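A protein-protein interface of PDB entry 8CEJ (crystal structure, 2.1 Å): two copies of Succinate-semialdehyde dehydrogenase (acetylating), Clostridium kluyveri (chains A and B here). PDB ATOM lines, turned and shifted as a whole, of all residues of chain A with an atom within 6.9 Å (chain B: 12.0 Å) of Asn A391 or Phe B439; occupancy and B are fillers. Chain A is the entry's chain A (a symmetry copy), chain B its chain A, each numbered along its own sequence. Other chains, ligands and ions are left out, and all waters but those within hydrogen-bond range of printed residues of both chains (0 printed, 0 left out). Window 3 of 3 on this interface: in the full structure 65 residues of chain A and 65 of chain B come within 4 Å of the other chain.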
ATOM      1  N   TYR A 221      -8.097 -23.265  20.210  1.00  0.00           N
ATOM      2  CA  TYR A 221      -6.770 -23.853  20.125  1.00  0.00           C
ATOM      3  C   TYR A 221      -6.712 -24.880  18.994  1.00  0.00           C
ATOM      4  O   TYR A 221      -7.735 -25.337  18.480  1.00  0.00           O
ATOM      5  CB  TYR A 221      -6.394 -24.502  21.460  1.00  0.00           C
ATOM      6  CG  TYR A 221      -4.965 -24.999  21.548  1.00  0.00           C
ATOM      7  CD1 TYR A 221      -3.915 -24.119  21.771  1.00  0.00           C
ATOM      8  CD2 TYR A 221      -4.671 -26.351  21.422  1.00  0.00           C
ATOM      9  CE1 TYR A 221      -2.613 -24.570  21.856  1.00  0.00           C
ATOM     10  CE2 TYR A 221      -3.372 -26.809  21.501  1.00  0.00           C
ATOM     11  CZ  TYR A 221      -2.347 -25.917  21.722  1.00  0.00           C
ATOM     12  OH  TYR A 221      -1.052 -26.370  21.805  1.00  0.00           O
ATOM     13  N   LYS A 225      -3.382 -30.533  17.425  1.00  0.00           N
ATOM     14  CA  LYS A 225      -2.183 -30.576  18.256  1.00  0.00           C
ATOM     15  C   LYS A 225      -2.512 -31.028  19.673  1.00  0.00           C
ATOM     16  O   LYS A 225      -1.789 -31.848  20.252  1.00  0.00           O
ATOM     17  CB  LYS A 225      -1.508 -29.205  18.271  1.00  0.00           C
ATOM     18  CG  LYS A 225      -0.270 -29.135  19.146  1.00  0.00           C
ATOM     19  CD  LYS A 225       0.791 -30.115  18.677  1.00  0.00           C
ATOM     20  CE  LYS A 225       1.985 -30.117  19.614  1.00  0.00           C
ATOM     21  NZ  LYS A 225       2.567 -28.755  19.765  1.00  0.00           N
ATOM     22  N   ASP A 229      -0.989 -34.432  21.610  1.00  0.00           N
ATOM     23  CA  ASP A 229      -0.265 -34.371  22.877  1.00  0.00           C
ATOM     24  C   ASP A 229      -0.962 -35.191  23.957  1.00  0.00           C
ATOM     25  O   ASP A 229      -0.300 -35.884  24.738  1.00  0.00           O
ATOM     26  CB  ASP A 229      -0.111 -32.917  23.324  1.00  0.00           C
ATOM     27  CG  ASP A 229       0.934 -32.168  22.522  1.00  0.00           C
ATOM     28  OD1 ASP A 229       1.646 -32.808  21.721  1.00  0.00           O
ATOM     29  OD2 ASP A 229       1.046 -30.935  22.695  1.00  0.00           O
ATOM     30  N   GLY A 367      -3.093 -30.424  32.913  1.00  0.00           N
ATOM     31  CA  GLY A 367      -2.663 -30.057  31.580  1.00  0.00           C
ATOM     32  C   GLY A 367      -3.652 -29.102  30.949  1.00  0.00           C
ATOM     33  O   GLY A 367      -4.857 -29.180  31.180  1.00  0.00           O
ATOM     34  N   ILE A 368      -3.120 -28.178  30.155  1.00  0.00           N
ATOM     35  CA  ILE A 368      -3.944 -27.205  29.451  1.00  0.00           C
ATOM     36  C   ILE A 368      -3.355 -26.981  28.067  1.00  0.00           C
ATOM     37  O   ILE A 368      -2.133 -27.022  27.882  1.00  0.00           O
ATOM     38  CB  ILE A 368      -4.064 -25.875  30.231  1.00  0.00           C
ATOM     39  CG1 ILE A 368      -5.131 -24.978  29.599  1.00  0.00           C
ATOM     40  CG2 ILE A 368      -2.722 -25.163  30.298  1.00  0.00           C
ATOM     41  CD1 ILE A 368      -5.467 -23.761  30.417  1.00  0.00           C
ATOM     42  N   HIS A 369      -4.233 -26.774  27.090  1.00  0.00           N
ATOM     43  CA  HIS A 369      -3.844 -26.504  25.708  1.00  0.00           C
ATOM     44  C   HIS A 369      -4.594 -25.249  25.277  1.00  0.00           C
ATOM     45  O   HIS A 369      -5.790 -25.305  24.977  1.00  0.00           O
ATOM     46  CB  HIS A 369      -4.151 -27.693  24.807  1.00  0.00           C
ATOM     47  CG  HIS A 369      -3.397 -28.932  25.173  1.00  0.00           C
ATOM     48  ND1 HIS A 369      -2.316 -29.385  24.448  1.00  0.00           N
ATOM     49  CD2 HIS A 369      -3.554 -29.801  26.199  1.00  0.00           C
ATOM     50  CE1 HIS A 369      -1.847 -30.486  25.006  1.00  0.00           C
ATOM     51  NE2 HIS A 369      -2.580 -30.760  26.070  1.00  0.00           N
ATOM     52  N   SER A 370      -3.893 -24.119  25.266  1.00  0.00           N
ATOM     53  CA  SER A 370      -4.533 -22.836  25.026  1.00  0.00           C
ATOM     54  C   SER A 370      -3.499 -21.834  24.538  1.00  0.00           C
ATOM     55  O   SER A 370      -2.318 -21.921  24.884  1.00  0.00           O
ATOM     56  CB  SER A 370      -5.214 -22.310  26.294  1.00  0.00           C
ATOM     57  OG  SER A 370      -5.729 -21.007  26.093  1.00  0.00           O
ATOM     58  N   ASP A 371      -3.962 -20.888  23.726  1.00  0.00           N
ATOM     59  CA  ASP A 371      -3.183 -19.719  23.347  1.00  0.00           C
ATOM     60  C   ASP A 371      -3.561 -18.486  24.156  1.00  0.00           C
ATOM     61  O   ASP A 371      -2.973 -17.421  23.952  1.00  0.00           O
ATOM     62  CB  ASP A 371      -3.353 -19.428  21.852  1.00  0.00           C
ATOM     63  CG  ASP A 371      -2.741 -20.503  20.975  1.00  0.00           C
ATOM     64  OD1 ASP A 371      -1.581 -20.892  21.229  1.00  0.00           O
ATOM     65  OD2 ASP A 371      -3.424 -20.962  20.036  1.00  0.00           O
ATOM     66  N   ILE A 376      -4.754 -19.461  30.929  1.00  0.00           N
ATOM     67  CA  ILE A 376      -3.756 -20.356  31.509  1.00  0.00           C
ATOM     68  C   ILE A 376      -3.418 -19.928  32.930  1.00  0.00           C
ATOM     69  O   ILE A 376      -3.310 -20.762  33.838  1.00  0.00           O
ATOM     70  CB  ILE A 376      -2.501 -20.400  30.617  1.00  0.00           C
ATOM     71  CG1 ILE A 376      -2.843 -20.986  29.246  1.00  0.00           C
ATOM     72  CG2 ILE A 376      -1.395 -21.200  31.285  1.00  0.00           C
ATOM     73  CD1 ILE A 376      -1.730 -20.858  28.235  1.00  0.00           C
ATOM     74  N   VAL A 389       0.826 -27.990  33.035  1.00  0.00           N
ATOM     75  CA  VAL A 389       1.597 -28.287  31.833  1.00  0.00           C
ATOM     76  C   VAL A 389       0.848 -27.704  30.642  1.00  0.00           C
ATOM     77  O   VAL A 389      -0.325 -28.027  30.419  1.00  0.00           O
ATOM     78  CB  VAL A 389       1.826 -29.798  31.673  1.00  0.00           C
ATOM     79  CG1 VAL A 389       2.824 -30.068  30.575  1.00  0.00           C
ATOM     80  CG2 VAL A 389       2.309 -30.399  32.987  1.00  0.00           C
ATOM     81  N   VAL A 390       1.525 -26.852  29.876  1.00  0.00           N
ATOM     82  CA  VAL A 390       0.890 -26.017  28.862  1.00  0.00           C
ATOM     83  C   VAL A 390       1.352 -26.462  27.481  1.00  0.00           C
ATOM     84  O   VAL A 390       2.550 -26.416  27.174  1.00  0.00           O
ATOM     85  CB  VAL A 390       1.205 -24.530  29.082  1.00  0.00           C
ATOM     86  CG1 VAL A 390       0.519 -23.684  28.023  1.00  0.00           C
ATOM     87  CG2 VAL A 390       0.788 -24.098  30.480  1.00  0.00           C
ATOM     88  N   ASN A 391       0.394 -26.876  26.646  1.00  0.00           N
ATOM     89  CA  ASN A 391       0.625 -27.138  25.221  1.00  0.00           C
ATOM     90  C   ASN A 391       1.687 -28.213  25.003  1.00  0.00           C
ATOM     91  O   ASN A 391       2.560 -28.084  24.141  1.00  0.00           O
ATOM     92  CB  ASN A 391       0.995 -25.852  24.481  1.00  0.00           C
ATOM     93  CG  ASN A 391      -0.117 -24.824  24.508  1.00  0.00           C
ATOM     94  OD1 ASN A 391      -1.082 -24.959  25.258  1.00  0.00           O
ATOM     95  ND2 ASN A 391       0.014 -23.786  23.694  1.00  0.00           N
ATOM     96  N   GLN A 392       1.602 -29.285  25.779  1.00  0.00           N
ATOM     97  CA  GLN A 392       2.515 -30.417  25.685  1.00  0.00           C
ATOM     98  C   GLN A 392       1.935 -31.558  26.517  1.00  0.00           C
ATOM     99  O   GLN A 392       1.064 -31.325  27.359  1.00  0.00           O
ATOM    100  CB  GLN A 392       3.927 -30.043  26.173  1.00  0.00           C
ATOM    101  CG  GLN A 392       3.945 -29.197  27.428  1.00  0.00           C
ATOM    102  CD  GLN A 392       5.343 -28.806  27.862  1.00  0.00           C
ATOM    103  OE1 GLN A 392       6.328 -29.426  27.462  1.00  0.00           O
ATOM    104  NE2 GLN A 392       5.436 -27.769  28.685  1.00  0.00           N
ATOM    105  N   PRO A 393       2.380 -32.795  26.280  1.00  0.00           N
ATOM    106  CA  PRO A 393       1.873 -33.917  27.079  1.00  0.00           C
ATOM    107  C   PRO A 393       2.140 -33.714  28.562  1.00  0.00           C
ATOM    108  O   PRO A 393       3.217 -33.268  28.963  1.00  0.00           O
ATOM    109  CB  PRO A 393       2.645 -35.121  26.527  1.00  0.00           C
ATOM    110  CG  PRO A 393       3.009 -34.730  25.145  1.00  0.00           C
ATOM    111  CD  PRO A 393       3.264 -33.253  25.192  1.00  0.00           C
ATOM    112  N   THR A 396       5.247 -34.952  30.647  1.00  0.00           N
ATOM    113  CA  THR A 396       6.495 -34.205  30.730  1.00  0.00           C
ATOM    114  C   THR A 396       6.636 -33.443  32.041  1.00  0.00           C
ATOM    115  O   THR A 396       7.632 -32.732  32.220  1.00  0.00           O
ATOM    116  CB  THR A 396       6.604 -33.227  29.557  1.00  0.00           C
ATOM    117  OG1 THR A 396       5.590 -32.222  29.676  1.00  0.00           O
ATOM    118  CG2 THR A 396       6.430 -33.956  28.235  1.00  0.00           C
ATOM    119  N   SER A 400      11.619 -32.279  31.248  1.00  0.00           N
ATOM    120  CA  SER A 400      11.824 -32.425  29.817  1.00  0.00           C
ATOM    121  C   SER A 400      12.873 -31.422  29.363  1.00  0.00           C
ATOM    122  O   SER A 400      13.125 -30.412  30.024  1.00  0.00           O
ATOM    123  CB  SER A 400      10.519 -32.221  29.032  1.00  0.00           C
ATOM    124  OG  SER A 400      10.759 -32.188  27.636  1.00  0.00           O
ATOM    125  N   ASN A 402      12.416 -29.509  27.039  1.00  0.00           N
ATOM    126  CA  ASN A 402      11.664 -28.404  26.456  1.00  0.00           C
ATOM    127  C   ASN A 402      10.773 -27.696  27.470  1.00  0.00           C
ATOM    128  O   ASN A 402       9.960 -26.851  27.076  1.00  0.00           O
ATOM    129  CB  ASN A 402      10.821 -28.901  25.277  1.00  0.00           C
ATOM    130  CG  ASN A 402      11.664 -29.507  24.172  1.00  0.00           C
ATOM    131  OD1 ASN A 402      12.175 -28.798  23.305  1.00  0.00           O
ATOM    132  ND2 ASN A 402      11.813 -30.827  24.194  1.00  0.00           N
ATOM    133  N   ASN A 403      10.890 -28.016  28.757  1.00  0.00           N
ATOM    134  CA  ASN A 403      10.165 -27.300  29.798  1.00  0.00           C
ATOM    135  C   ASN A 403      11.083 -27.092  30.995  1.00  0.00           C
ATOM    136  O   ASN A 403      12.176 -27.660  31.076  1.00  0.00           O
ATOM    137  CB  ASN A 403       8.872 -28.027  30.207  1.00  0.00           C
ATOM    138  CG  ASN A 403       9.110 -29.450  30.686  1.00  0.00           C
ATOM    139  OD1 ASN A 403      10.187 -29.794  31.171  1.00  0.00           O
ATOM    140  ND2 ASN A 403       8.090 -30.289  30.554  1.00  0.00           N
ATOM    141  N   GLU B  90       9.618 -16.583  35.749  1.00  0.00           N
ATOM    142  CA  GLU B  90      10.970 -16.962  35.347  1.00  0.00           C
ATOM    143  C   GLU B  90      10.945 -17.299  33.861  1.00  0.00           C
ATOM    144  O   GLU B  90      10.872 -18.478  33.480  1.00  0.00           O
ATOM    145  CB  GLU B  90      11.484 -18.135  36.179  1.00  0.00           C
ATOM    146  CG  GLU B  90      12.956 -18.436  35.983  1.00  0.00           C
ATOM    147  CD  GLU B  90      13.477 -19.460  36.969  1.00  0.00           C
ATOM    148  OE1 GLU B  90      12.659 -20.042  37.712  1.00  0.00           O
ATOM    149  OE2 GLU B  90      14.706 -19.679  37.004  1.00  0.00           O
ATOM    150  N   PRO B  91      11.001 -16.287  32.990  1.00  0.00           N
ATOM    151  CA  PRO B  91      10.915 -16.565  31.547  1.00  0.00           C
ATOM    152  C   PRO B  91      12.092 -17.359  31.010  1.00  0.00           C
ATOM    153  O   PRO B  91      11.940 -18.049  29.995  1.00  0.00           O
ATOM    154  CB  PRO B  91      10.845 -15.163  30.925  1.00  0.00           C
ATOM    155  CG  PRO B  91      11.472 -14.267  31.939  1.00  0.00           C
ATOM    156  CD  PRO B  91      11.111 -14.847  33.274  1.00  0.00           C
ATOM    157  N   GLU B  92      13.260 -17.290  31.652  1.00  0.00           N
ATOM    158  CA  GLU B  92      14.402 -18.064  31.179  1.00  0.00           C
ATOM    159  C   GLU B  92      14.185 -19.562  31.337  1.00  0.00           C
ATOM    160  O   GLU B  92      14.812 -20.345  30.615  1.00  0.00           O
ATOM    161  CB  GLU B  92      15.681 -17.636  31.904  1.00  0.00           C
ATOM    162  CG  GLU B  92      15.638 -17.758  33.421  1.00  0.00           C
ATOM    163  CD  GLU B  92      15.063 -16.526  34.097  1.00  0.00           C
ATOM    164  OE1 GLU B  92      14.297 -15.785  33.445  1.00  0.00           O
ATOM    165  OE2 GLU B  92      15.379 -16.298  35.284  1.00  0.00           O
ATOM    166  N   ARG B  93      13.315 -19.979  32.256  1.00  0.00           N
ATOM    167  CA  ARG B  93      12.924 -21.376  32.382  1.00  0.00           C
ATOM    168  C   ARG B  93      11.507 -21.635  31.895  1.00  0.00           C
ATOM    169  O   ARG B  93      11.020 -22.762  32.027  1.00  0.00           O
ATOM    170  CB  ARG B  93      13.053 -21.845  33.838  1.00  0.00           C
ATOM    171  CG  ARG B  93      14.456 -21.761  34.409  1.00  0.00           C
ATOM    172  CD  ARG B  93      14.577 -22.610  35.666  1.00  0.00           C
ATOM    173  NE  ARG B  93      14.595 -24.036  35.360  1.00  0.00           N
ATOM    174  CZ  ARG B  93      14.541 -25.001  36.269  1.00  0.00           C
ATOM    175  NH1 ARG B  93      14.437 -24.729  37.560  1.00  0.00           N
ATOM    176  NH2 ARG B  93      14.591 -26.269  35.872  1.00  0.00           N
ATOM    177  N   ALA B  94      10.839 -20.625  31.334  1.00  0.00           N
ATOM    178  CA  ALA B  94       9.444 -20.728  30.907  1.00  0.00           C
ATOM    179  C   ALA B  94       8.558 -21.194  32.062  1.00  0.00           C
ATOM    180  O   ALA B  94       7.727 -22.093  31.922  1.00  0.00           O
ATOM    181  CB  ALA B  94       9.304 -21.650  29.694  1.00  0.00           C
ATOM    182  N   LEU B  95       8.748 -20.566  33.218  1.00  0.00           N
ATOM    183  CA  LEU B  95       8.062 -20.934  34.447  1.00  0.00           C
ATOM    184  C   LEU B  95       7.319 -19.739  35.022  1.00  0.00           C
ATOM    185  O   LEU B  95       7.796 -18.602  34.952  1.00  0.00           O
ATOM    186  CB  LEU B  95       9.045 -21.466  35.495  1.00  0.00           C
ATOM    187  CG  LEU B  95       9.521 -22.911  35.363  1.00  0.00           C
ATOM    188  CD1 LEU B  95      10.501 -23.239  36.473  1.00  0.00           C
ATOM    189  CD2 LEU B  95       8.337 -23.857  35.402  1.00  0.00           C
ATOM    190  N   VAL B  96       6.147 -20.007  35.594  1.00  0.00           N
ATOM    191  CA  VAL B  96       5.397 -19.035  36.376  1.00  0.00           C
ATOM    192  C   VAL B  96       5.081 -19.674  37.720  1.00  0.00           C
ATOM    193  O   VAL B  96       4.541 -20.784  37.770  1.00  0.00           O
ATOM    194  CB  VAL B  96       4.104 -18.589  35.667  1.00  0.00           C
ATOM    195  CG1 VAL B  96       3.377 -17.551  36.503  1.00  0.00           C
ATOM    196  CG2 VAL B  96       4.414 -18.039  34.286  1.00  0.00           C
ATOM    197  N   ARG B 435       3.960 -24.506  39.637  1.00  0.00           N
ATOM    198  CA  ARG B 435       4.632 -24.045  38.432  1.00  0.00           C
ATOM    199  C   ARG B 435       3.723 -24.236  37.228  1.00  0.00           C
ATOM    200  O   ARG B 435       3.017 -25.243  37.126  1.00  0.00           O
ATOM    201  CB  ARG B 435       5.957 -24.788  38.221  1.00  0.00           C
ATOM    202  CG  ARG B 435       7.021 -24.444  39.251  1.00  0.00           C
ATOM    203  CD  ARG B 435       8.130 -25.480  39.285  1.00  0.00           C
ATOM    204  NE  ARG B 435       9.186 -25.111  40.219  1.00  0.00           N
ATOM    205  CZ  ARG B 435       9.126 -25.295  41.530  1.00  0.00           C
ATOM    206  NH1 ARG B 435       8.067 -25.840  42.105  1.00  0.00           N
ATOM    207  NH2 ARG B 435      10.155 -24.919  42.286  1.00  0.00           N
ATOM    208  N   ILE B 436       3.751 -23.263  36.316  1.00  0.00           N
ATOM    209  CA  ILE B 436       2.903 -23.297  35.128  1.00  0.00           C
ATOM    210  C   ILE B 436       3.642 -23.817  33.893  1.00  0.00           C
ATOM    211  O   ILE B 436       2.984 -24.241  32.930  1.00  0.00           O
ATOM    212  CB  ILE B 436       2.295 -21.900  34.867  1.00  0.00           C
ATOM    213  CG1 ILE B 436       1.578 -21.407  36.125  1.00  0.00           C
ATOM    214  CG2 ILE B 436       1.307 -21.923  33.709  1.00  0.00           C
ATOM    215  CD1 ILE B 436       0.668 -20.220  35.894  1.00  0.00           C
ATOM    216  N   GLY B 437       4.975 -23.807  33.897  1.00  0.00           N
ATOM    217  CA  GLY B 437       5.801 -24.493  32.912  1.00  0.00           C
ATOM    218  C   GLY B 437       5.326 -24.526  31.472  1.00  0.00           C
ATOM    219  O   GLY B 437       4.594 -25.437  31.073  1.00  0.00           O
ATOM    220  N   TYR B 438       5.751 -23.552  30.674  1.00  0.00           N
ATOM    221  CA  TYR B 438       5.332 -23.481  29.285  1.00  0.00           C
ATOM    222  C   TYR B 438       6.210 -24.380  28.416  1.00  0.00           C
ATOM    223  O   TYR B 438       7.176 -24.993  28.877  1.00  0.00           O
ATOM    224  CB  TYR B 438       5.366 -22.035  28.798  1.00  0.00           C
ATOM    225  CG  TYR B 438       4.276 -21.179  29.394  1.00  0.00           C
ATOM    226  CD1 TYR B 438       4.388 -20.681  30.684  1.00  0.00           C
ATOM    227  CD2 TYR B 438       3.133 -20.875  28.669  1.00  0.00           C
ATOM    228  CE1 TYR B 438       3.393 -19.901  31.236  1.00  0.00           C
ATOM    229  CE2 TYR B 438       2.132 -20.095  29.212  1.00  0.00           C
ATOM    230  CZ  TYR B 438       2.268 -19.611  30.495  1.00  0.00           C
ATOM    231  OH  TYR B 438       1.273 -18.834  31.041  1.00  0.00           O
ATOM    232  N   PHE B 439       5.862 -24.460  27.134  1.00  0.00           N
ATOM    233  CA  PHE B 439       6.591 -25.281  26.174  1.00  0.00           C
ATOM    234  C   PHE B 439       7.691 -24.432  25.546  1.00  0.00           C
ATOM    235  O   PHE B 439       7.414 -23.551  24.726  1.00  0.00           O
ATOM    236  CB  PHE B 439       5.641 -25.832  25.114  1.00  0.00           C
ATOM    237  CG  PHE B 439       6.287 -26.797  24.160  1.00  0.00           C
ATOM    238  CD1 PHE B 439       6.475 -28.120  24.517  1.00  0.00           C
ATOM    239  CD2 PHE B 439       6.697 -26.382  22.904  1.00  0.00           C
ATOM    240  CE1 PHE B 439       7.066 -29.012  23.642  1.00  0.00           C
ATOM    241  CE2 PHE B 439       7.287 -27.269  22.024  1.00  0.00           C
ATOM    242  CZ  PHE B 439       7.473 -28.586  22.394  1.00  0.00           C
ATOM    243  N   ASN B 440       8.937 -24.696  25.932  1.00  0.00           N
ATOM    244  CA  ASN B 440      10.079 -23.940  25.427  1.00  0.00           C
ATOM    245  C   ASN B 440      10.506 -24.536  24.091  1.00  0.00           C
ATOM    246  O   ASN B 440      11.001 -25.666  24.036  1.00  0.00           O
ATOM    247  CB  ASN B 440      11.221 -23.962  26.438  1.00  0.00           C
ATOM    248  CG  ASN B 440      12.220 -22.840  26.218  1.00  0.00           C
ATOM    249  OD1 ASN B 440      12.473 -22.429  25.085  1.00  0.00           O
ATOM    250  ND2 ASN B 440      12.793 -22.337  27.308  1.00  0.00           N
ATOM    251  N   LYS B 441      10.316 -23.776  23.013  1.00  0.00           N
ATOM    252  CA  LYS B 441      10.623 -24.257  21.672  1.00  0.00           C
ATOM    253  C   LYS B 441      12.034 -23.897  21.225  1.00  0.00           C
ATOM    254  O   LYS B 441      12.626 -24.625  20.418  1.00  0.00           O
ATOM    255  CB  LYS B 441       9.604 -23.697  20.674  1.00  0.00           C
ATOM    256  CG  LYS B 441       9.669 -24.311  19.285  1.00  0.00           C
ATOM    257  CD  LYS B 441       8.620 -23.696  18.373  1.00  0.00           C
ATOM    258  CE  LYS B 441       8.708 -24.258  16.965  1.00  0.00           C
ATOM    259  NZ  LYS B 441       7.701 -23.637  16.061  1.00  0.00           N
ATOM    260  N   GLU B 442      12.591 -22.795  21.734  1.00  0.00           N
ATOM    261  CA  GLU B 442      13.937 -22.391  21.344  1.00  0.00           C
ATOM    262  C   GLU B 442      15.009 -23.322  21.895  1.00  0.00           C
ATOM    263  O   GLU B 442      16.131 -23.328  21.378  1.00  0.00           O
ATOM    264  CB  GLU B 442      14.213 -20.957  21.805  1.00  0.00           C
ATOM    265  CG  GLU B 442      13.320 -19.910  21.161  1.00  0.00           C
ATOM    266  CD  GLU B 442      13.705 -18.497  21.554  1.00  0.00           C
ATOM    267  OE1 GLU B 442      14.669 -18.336  22.331  1.00  0.00           O
ATOM    268  OE2 GLU B 442      13.043 -17.546  21.087  1.00  0.00           O
ATOM    269  N   ALA B 443      14.694 -24.101  22.927  1.00  0.00           N
ATOM    270  CA  ALA B 443      15.679 -25.002  23.510  1.00  0.00           C
ATOM    271  C   ALA B 443      15.993 -26.145  22.554  1.00  0.00           C
ATOM    272  O   ALA B 443      15.103 -26.691  21.895  1.00  0.00           O
ATOM    273  CB  ALA B 443      15.172 -25.551  24.843  1.00  0.00           C
ATOM    274  N   LYS B 444      17.271 -26.505  22.481  1.00  0.00           N
ATOM    275  CA  LYS B 444      17.738 -27.582  21.620  1.00  0.00           C
ATOM    276  C   LYS B 444      17.973 -28.840  22.445  1.00  0.00           C
ATOM    277  O   LYS B 444      18.561 -28.784  23.529  1.00  0.00           O
ATOM    278  CB  LYS B 444      19.025 -27.183  20.895  1.00  0.00           C
ATOM    279  CG  LYS B 444      18.904 -25.910  20.073  1.00  0.00           C
ATOM    280  CD  LYS B 444      17.826 -26.038  19.010  1.00  0.00           C
ATOM    281  CE  LYS B 444      17.681 -24.754  18.212  1.00  0.00           C
ATOM    282  NZ  LYS B 444      16.622 -24.864  17.172  1.00  0.00           N
ATOM    283  N   VAL B 445      17.511 -29.973  21.925  1.00  0.00           N
ATOM    284  CA  VAL B 445      17.649 -31.254  22.615  1.00  0.00           C
ATOM    285  C   VAL B 445      19.101 -31.712  22.541  1.00  0.00           C
ATOM    286  O   VAL B 445      19.642 -31.885  21.438  1.00  0.00           O
ATOM    287  CB  VAL B 445      16.696 -32.309  22.030  1.00  0.00           C
ATOM    288  CG1 VAL B 445      16.674 -32.230  20.507  1.00  0.00           C
ATOM    289  CG2 VAL B 445      17.098 -33.702  22.495  1.00  0.00           C
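O of Gly B437 sits at hydrogen-bond distance from NE2 of Gln A392 (3.4 Å). The side-chain amide nitrogen (NE2) of Gln A392 sits at hydrogen-bond distance from the backbone carbonyl oxygen (O) of Tyr B438, 3.3 Å away. The backbone NH (N) of Asn B440 sits at hydrogen-bond distance from the backbone carbonyl oxygen (O) of Asn A402 (2.6 Å).
The backbone carbonyl oxygen (O) of Ala B94 lies within hydrogen-bond range of the backbone NH (N) of Tyr B438, at 2.8 Å. N of Ile B436 lies within hydrogen-bond range of O of Val B96. OH of Tyr A221 lies close to ND2 of Asn A391. The backbone carbonyl oxygen (O) of Ile A368 sits at hydrogen-bond distance from the backbone NH (N) of Asn A391, at 2.8 Å. The backbone NH of Ser A370 is in hydrogen-bond range of the side-chain amide oxygen of Asn A391, 2.9 Å away. N of Asn A402 sits close to OG of Ser A400.
Ile B436 touches Ile A376. Ile A376 touches Tyr B438. Val A390 touches Ile B436 (CG2 to O, 3.3 Å). N of Val A390 touches O of Gly B437, at 3.6 Å. CG1 of Val A390 touches CD2 of Tyr B438, 3.9 Å away. Phe B439 touches Val A390. O of Asn A391 touches CD1 of Phe B439, at 3.9 Å. O of Tyr B438 touches O of Asn A402 (3.8 Å). Asn A402 touches Phe B439. O of Tyr B438 touches CB of Asn A403, at 3.7 Å.
Asp A229 touches none of the printed residues of chain B. Ile A368 touches none of the printed residues of chain B. Asp A371 touches none of the printed residues of chain B. Of the printed residues of chain B, Ile A376 touches Ile B436 and Tyr B438. No residue of chain B comes within 4 Å of Val A389. Asn A391 touches one residue of chain B. Gln A392 touches three residues of chain B. Ser A400 touches none of the printed residues of chain B. Of chain B, only Tyr B438, Phe B439, Asn B440 and Ala B443 come within 4 Å of Asn A402. Glu B90 touches none of the printed residues of chain A. Of chain A, only Val A390, Asn A391, Gln A392 and Asn A402 come within 4 Å of Phe B439. Of the printed residues of chain A, Ala B443 touches Asn A402. The nearest residue of chain A that does not touch Phe B439 is Asn A403 (5.4 Å).
Hydrophobic or aromatic side chains of chain A that line the printed part of chain B: Ile A376 and Val A390. Of the 18 printed residues of chain B, 6 touch a printed residue of chain A. Among the printed residues, 15 pairs touch across the chains.
No position is printed for both chains. Of the 15 pairs that touch across the chains among the printed residues, none has its exchanged pair printed and touching as well.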
